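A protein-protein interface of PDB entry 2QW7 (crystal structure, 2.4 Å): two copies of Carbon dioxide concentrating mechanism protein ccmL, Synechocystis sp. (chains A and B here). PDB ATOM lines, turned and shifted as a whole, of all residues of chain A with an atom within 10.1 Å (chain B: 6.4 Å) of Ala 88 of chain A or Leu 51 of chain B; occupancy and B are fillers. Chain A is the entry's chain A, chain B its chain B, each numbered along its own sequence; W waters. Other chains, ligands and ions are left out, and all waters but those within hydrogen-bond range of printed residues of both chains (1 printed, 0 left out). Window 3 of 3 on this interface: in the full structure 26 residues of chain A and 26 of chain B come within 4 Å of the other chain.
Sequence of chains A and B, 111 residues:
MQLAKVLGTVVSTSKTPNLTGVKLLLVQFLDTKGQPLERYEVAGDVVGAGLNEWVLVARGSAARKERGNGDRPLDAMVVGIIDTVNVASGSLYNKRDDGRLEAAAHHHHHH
The backbone carbonyl oxygen (O) of Val 85 of chain A is in hydrogen-bond range of the backbone NH (N) of Leu 92 of chain A (2.6 Å). The backbone carbonyl oxygen (O) of Tyr 93 of chain A is in hydrogen-bond range of the backbone NH (N) of Val 85 of chain A, at 2.9 Å. The side-chain amide nitrogen (ND2) of Asn 86 of chain A is in hydrogen-bond range of the side-chain hydroxyl (OG) of Ser 91 of chain A.
Printed residues of chain B that touch a printed residue of chain A: Leu 7, Gly 8, Thr 9 and Leu 51. Hydrophobic or aromatic side chains of chain B within 4 Å of the printed part of chain A: Leu 7 and Leu 51. Of the 10 printed residues of chain A, 5 touch a printed residue of chain B. Printed residues of chain A that touch a printed residue of chain B: Thr 32, Val 85, Asn 86, Val 87 and Ala 88. Hydrophobic or aromatic side chains of chain A within 4 Å of the printed part of chain B: Val 87 and Ala 88. Among the printed residues, 7 pairs touch across the chains.
Water W1 lies within hydrogen-bond range of O of Leu 7 of chain B and N of Ala 88 of chain A.
Of the printed residues of chain B, Thr 32 of chain A touches Leu 7 (3.8 Å). Printed residues of chain B within 4 Å of Asn 86 of chain A: Gly 8 (3.0 Å) and Thr 9 (3.0 Å). Printed residues of chain B within 4 Å of Val 87 of chain A: Leu 7 (3.4 Å). Of chain B, only Leu 7 and Leu 51 come within 4 Å of Ala 88 of chain A. No residue of chain A comes within 4 Å of Gly 50 of chain B. Of the printed residues of chain A, Leu 51 of chain B touches Ala 88 (3.6 Å). Glu 53 of chain B touches none of the printed residues of chain A. The nearest printed residue of chain B that does not touch Ala 88 of chain A is Gly 8 of chain B (5.6 Å). The nearest printed residue of chain A that does not touch Leu 7 of chain B is Asn 86 of chain A (4.1 Å).
The backbone NH of Thr 9 of chain B sits at hydrogen-bond distance from the backbone carbonyl oxygen of Asn 86 of chain A, at 3.0 Å.
Among the printed residues, merely in contact across the chains: Asn 86 of chain A with Gly 8 of chain B, Val 87 of chain A with Leu 7 of chain B, Ala 88 of chain A with Leu 51 of chain B, Ala 88 of chain A with Leu 7 of chain B, Val 85 of chain A with Thr 9 of chain B and Thr 32 of chain A with Leu 7 of chain B.
No position is printed for both chains.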
ATOM      1  N   THR A  32     -15.400  -4.838 -20.684  1.00  0.00           N
ATOM      2  CA  THR A  32     -15.123  -3.857 -19.614  1.00  0.00           C
ATOM      3  C   THR A  32     -15.172  -4.488 -18.221  1.00  0.00           C
ATOM      4  O   THR A  32     -14.769  -3.853 -17.261  1.00  0.00           O
ATOM      5  CB  THR A  32     -16.087  -2.645 -19.515  1.00  0.00           C
ATOM      6  OG1 THR A  32     -17.409  -3.130 -19.280  1.00  0.00           O
ATOM      7  CG2 THR A  32     -16.045  -1.766 -20.751  1.00  0.00           C
ATOM      8  N   VAL A  85      -5.888  -2.088 -14.562  1.00  0.00           N
ATOM      9  CA  VAL A  85      -7.109  -1.456 -15.053  1.00  0.00           C
ATOM     10  C   VAL A  85      -7.880  -0.966 -13.826  1.00  0.00           C
ATOM     11  O   VAL A  85      -8.440  -1.777 -13.083  1.00  0.00           O
ATOM     12  CB  VAL A  85      -8.127  -2.376 -15.733  1.00  0.00           C
ATOM     13  CG1 VAL A  85      -9.260  -1.511 -16.225  1.00  0.00           C
ATOM     14  CG2 VAL A  85      -7.519  -3.191 -16.851  1.00  0.00           C
ATOM     15  N   ASN A  86      -7.954   0.361 -13.678  1.00  0.00           N
ATOM     16  CA  ASN A  86      -8.598   1.013 -12.530  1.00  0.00           C
ATOM     17  C   ASN A  86      -9.951   1.676 -12.857  1.00  0.00           C
ATOM     18  O   ASN A  86      -9.971   2.645 -13.649  1.00  0.00           O
ATOM     19  CB  ASN A  86      -7.649   2.118 -11.987  1.00  0.00           C
ATOM     20  CG  ASN A  86      -6.326   1.582 -11.366  1.00  0.00           C
ATOM     21  OD1 ASN A  86      -5.220   1.982 -11.760  1.00  0.00           O
ATOM     22  ND2 ASN A  86      -6.447   0.694 -10.405  1.00  0.00           N
ATOM     23  N   VAL A  87     -11.037   1.183 -12.241  1.00  0.00           N
ATOM     24  CA  VAL A  87     -12.378   1.725 -12.450  1.00  0.00           C
ATOM     25  C   VAL A  87     -12.879   2.507 -11.221  1.00  0.00           C
ATOM     26  O   VAL A  87     -12.104   2.819 -10.322  1.00  0.00           O
ATOM     27  CB  VAL A  87     -13.356   0.648 -12.946  1.00  0.00           C
ATOM     28  CG1 VAL A  87     -12.878   0.165 -14.302  1.00  0.00           C
ATOM     29  CG2 VAL A  87     -13.525  -0.499 -11.940  1.00  0.00           C
ATOM     30  N   ALA A  88     -14.160   2.873 -11.186  1.00  0.00           N
ATOM     31  CA  ALA A  88     -14.716   3.613 -10.029  1.00  0.00           C
ATOM     32  C   ALA A  88     -14.816   2.709  -8.803  1.00  0.00           C
ATOM     33  O   ALA A  88     -14.559   3.165  -7.690  1.00  0.00           O
ATOM     34  CB  ALA A  88     -16.088   4.237 -10.356  1.00  0.00           C
ATOM     35  N   SER A  89     -15.185   1.440  -9.004  1.00  0.00           N
ATOM     36  CA  SER A  89     -15.273   0.472  -7.901  1.00  0.00           C
ATOM     37  C   SER A  89     -13.900   0.194  -7.303  1.00  0.00           C
ATOM     38  O   SER A  89     -13.780  -0.204  -6.154  1.00  0.00           O
ATOM     39  CB  SER A  89     -15.850  -0.866  -8.375  1.00  0.00           C
ATOM     40  OG  SER A  89     -17.219  -0.771  -8.725  1.00  0.00           O
ATOM     41  N   GLY A  90     -12.867   0.371  -8.116  1.00  0.00           N
ATOM     42  CA  GLY A  90     -11.480   0.135  -7.724  1.00  0.00           C
ATOM     43  C   GLY A  90     -10.726  -0.549  -8.855  1.00  0.00           C
ATOM     44  O   GLY A  90     -11.038  -0.350 -10.031  1.00  0.00           O
ATOM     45  N   SER A  91      -9.743  -1.378  -8.521  1.00  0.00           N
ATOM     46  CA  SER A  91      -8.978  -2.072  -9.570  1.00  0.00           C
ATOM     47  C   SER A  91      -9.783  -3.244 -10.146  1.00  0.00           C
ATOM     48  O   SER A  91     -10.350  -4.075  -9.411  1.00  0.00           O
ATOM     49  CB  SER A  91      -7.594  -2.537  -9.127  1.00  0.00           C
ATOM     50  OG  SER A  91      -6.681  -1.456  -9.032  1.00  0.00           O
ATOM     51  N   LEU A  92      -9.881  -3.269 -11.470  1.00  0.00           N
ATOM     52  CA  LEU A  92     -10.578  -4.371 -12.158  1.00  0.00           C
ATOM     53  C   LEU A  92      -9.547  -5.450 -12.496  1.00  0.00           C
ATOM     54  O   LEU A  92      -9.842  -6.636 -12.605  1.00  0.00           O
ATOM     55  CB  LEU A  92     -11.383  -3.857 -13.355  1.00  0.00           C
ATOM     56  CG  LEU A  92     -12.067  -4.757 -14.379  1.00  0.00           C
ATOM     57  CD1 LEU A  92     -11.053  -5.216 -15.404  1.00  0.00           C
ATOM     58  CD2 LEU A  92     -12.846  -5.920 -13.738  1.00  0.00           C
ATOM     59  N   TYR A  93      -8.303  -5.002 -12.604  1.00  0.00           N
ATOM     60  CA  TYR A  93      -7.203  -5.876 -12.897  1.00  0.00           C
ATOM     61  C   TYR A  93      -5.895  -5.321 -12.375  1.00  0.00           C
ATOM     62  O   TYR A  93      -5.635  -4.130 -12.487  1.00  0.00           O
ATOM     63  CB  TYR A  93      -7.086  -6.032 -14.404  1.00  0.00           C
ATOM     64  CG  TYR A  93      -6.003  -6.972 -14.788  1.00  0.00           C
ATOM     65  CD1 TYR A  93      -4.788  -6.505 -15.378  1.00  0.00           C
ATOM     66  CD2 TYR A  93      -6.161  -8.327 -14.503  1.00  0.00           C
ATOM     67  CE1 TYR A  93      -3.793  -7.407 -15.714  1.00  0.00           C
ATOM     68  CE2 TYR A  93      -5.188  -9.230 -14.812  1.00  0.00           C
ATOM     69  CZ  TYR A  93      -4.011  -8.787 -15.412  1.00  0.00           C
ATOM     70  OH  TYR A  93      -3.114  -9.801 -15.685  1.00  0.00           O
ATOM     71  N   LYS B   5     -18.576   7.030 -21.973  1.00  0.00           N
ATOM     72  CA  LYS B   5     -18.476   7.450 -20.572  1.00  0.00           C
ATOM     73  C   LYS B   5     -17.152   6.949 -20.050  1.00  0.00           C
ATOM     74  O   LYS B   5     -16.780   5.798 -20.316  1.00  0.00           O
ATOM     75  CB  LYS B   5     -19.682   6.837 -19.787  1.00  0.00           C
ATOM     76  CG  LYS B   5     -19.634   6.959 -18.266  1.00  0.00           C
ATOM     77  CD  LYS B   5     -20.987   7.310 -17.624  1.00  0.00           C
ATOM     78  CE  LYS B   5     -20.807   7.625 -16.111  1.00  0.00           C
ATOM     79  NZ  LYS B   5     -21.841   8.500 -15.426  1.00  0.00           N
ATOM     80  N   VAL B   6     -16.422   7.793 -19.333  1.00  0.00           N
ATOM     81  CA  VAL B   6     -15.116   7.363 -18.831  1.00  0.00           C
ATOM     82  C   VAL B   6     -15.288   6.451 -17.602  1.00  0.00           C
ATOM     83  O   VAL B   6     -15.851   6.849 -16.583  1.00  0.00           O
ATOM     84  CB  VAL B   6     -14.163   8.492 -18.493  1.00  0.00           C
ATOM     85  CG1 VAL B   6     -12.845   7.896 -18.127  1.00  0.00           C
ATOM     86  CG2 VAL B   6     -14.018   9.446 -19.656  1.00  0.00           C
ATOM     87  N   LEU B   7     -14.823   5.215 -17.765  1.00  0.00           N
ATOM     88  CA  LEU B   7     -14.844   4.201 -16.730  1.00  0.00           C
ATOM     89  C   LEU B   7     -13.592   4.214 -15.846  1.00  0.00           C
ATOM     90  O   LEU B   7     -13.672   4.023 -14.644  1.00  0.00           O
ATOM     91  CB  LEU B   7     -15.121   2.818 -17.320  1.00  0.00           C
ATOM     92  CG  LEU B   7     -16.455   2.068 -17.078  1.00  0.00           C
ATOM     93  CD1 LEU B   7     -17.733   2.957 -17.152  1.00  0.00           C
ATOM     94  CD2 LEU B   7     -16.531   0.841 -18.024  1.00  0.00           C
ATOM     95  N   GLY B   8     -12.433   4.488 -16.411  1.00  0.00           N
ATOM     96  CA  GLY B   8     -11.240   4.552 -15.606  1.00  0.00           C
ATOM     97  C   GLY B   8     -10.032   4.716 -16.472  1.00  0.00           C
ATOM     98  O   GLY B   8     -10.172   5.255 -17.566  1.00  0.00           O
ATOM     99  N   THR B   9      -8.870   4.254 -15.961  1.00  0.00           N
ATOM    100  CA  THR B   9      -7.536   4.384 -16.620  1.00  0.00           C
ATOM    101  C   THR B   9      -6.776   3.063 -16.783  1.00  0.00           C
ATOM    102  O   THR B   9      -6.960   2.116 -15.995  1.00  0.00           O
ATOM    103  CB  THR B   9      -6.684   5.310 -15.813  1.00  0.00           C
ATOM    104  OG1 THR B   9      -7.109   6.653 -16.105  1.00  0.00           O
ATOM    105  CG2 THR B   9      -5.239   5.157 -16.216  1.00  0.00           C
ATOM    106  N   ALA B  49     -10.107  14.233 -20.062  1.00  0.00           N
ATOM    107  CA  ALA B  49     -11.368  13.725 -19.496  1.00  0.00           C
ATOM    108  C   ALA B  49     -11.211  13.007 -18.160  1.00  0.00           C
ATOM    109  O   ALA B  49     -10.197  12.381 -17.874  1.00  0.00           O
ATOM    110  CB  ALA B  49     -12.028  12.788 -20.453  1.00  0.00           C
ATOM    111  N   GLY B  50     -12.249  13.049 -17.353  1.00  0.00           N
ATOM    112  CA  GLY B  50     -12.214  12.435 -16.041  1.00  0.00           C
ATOM    113  C   GLY B  50     -13.324  11.407 -15.844  1.00  0.00           C
ATOM    114  O   GLY B  50     -14.238  11.306 -16.648  1.00  0.00           O
ATOM    115  N   LEU B  51     -13.233  10.657 -14.751  1.00  0.00           N
ATOM    116  CA  LEU B  51     -14.195   9.608 -14.436  1.00  0.00           C
ATOM    117  C   LEU B  51     -15.648  10.091 -14.579  1.00  0.00           C
ATOM    118  O   LEU B  51     -16.024  11.161 -14.107  1.00  0.00           O
ATOM    119  CB  LEU B  51     -13.954   9.027 -13.037  1.00  0.00           C
ATOM    120  CG  LEU B  51     -14.749   7.731 -12.808  1.00  0.00           C
ATOM    121  CD1 LEU B  51     -13.999   6.514 -13.359  1.00  0.00           C
ATOM    122  CD2 LEU B  51     -15.045   7.516 -11.290  1.00  0.00           C
ATOM    123  N   ASN B  52     -16.450   9.301 -15.269  1.00  0.00           N
ATOM    124  CA  ASN B  52     -17.882   9.586 -15.476  1.00  0.00           C
ATOM    125  C   ASN B  52     -18.309  10.628 -16.466  1.00  0.00           C
ATOM    126  O   ASN B  52     -19.501  10.744 -16.749  1.00  0.00           O
ATOM    127  CB  ASN B  52     -18.552  10.074 -14.203  1.00  0.00           C
ATOM    128  CG  ASN B  52     -18.586   9.057 -13.208  1.00  0.00           C
ATOM    129  OD1 ASN B  52     -18.821   7.900 -13.562  1.00  0.00           O
ATOM    130  ND2 ASN B  52     -18.355   9.434 -11.948  1.00  0.00           N
ATOM    131  N   GLU B  53     -17.350  11.412 -16.932  1.00  0.00           N
ATOM    132  CA  GLU B  53     -17.647  12.424 -17.927  1.00  0.00           C
ATOM    133  C   GLU B  53     -18.057  11.700 -19.203  1.00  0.00           C
ATOM    134  O   GLU B  53     -17.590  10.569 -19.447  1.00  0.00           O
ATOM    135  CB  GLU B  53     -16.449  13.360 -18.149  1.00  0.00           C
ATOM    136  CG  GLU B  53     -16.041  14.079 -16.840  1.00  0.00           C
ATOM    137  CD  GLU B  53     -15.059  15.251 -16.982  1.00  0.00           C
ATOM    138  OE1 GLU B  53     -14.889  15.841 -18.062  1.00  0.00           O
ATOM    139  OE2 GLU B  53     -14.445  15.634 -15.957  1.00  0.00           O
HETATM  140  O   HOH W   1     -15.819   2.699 -13.450  1.00  0.00           O
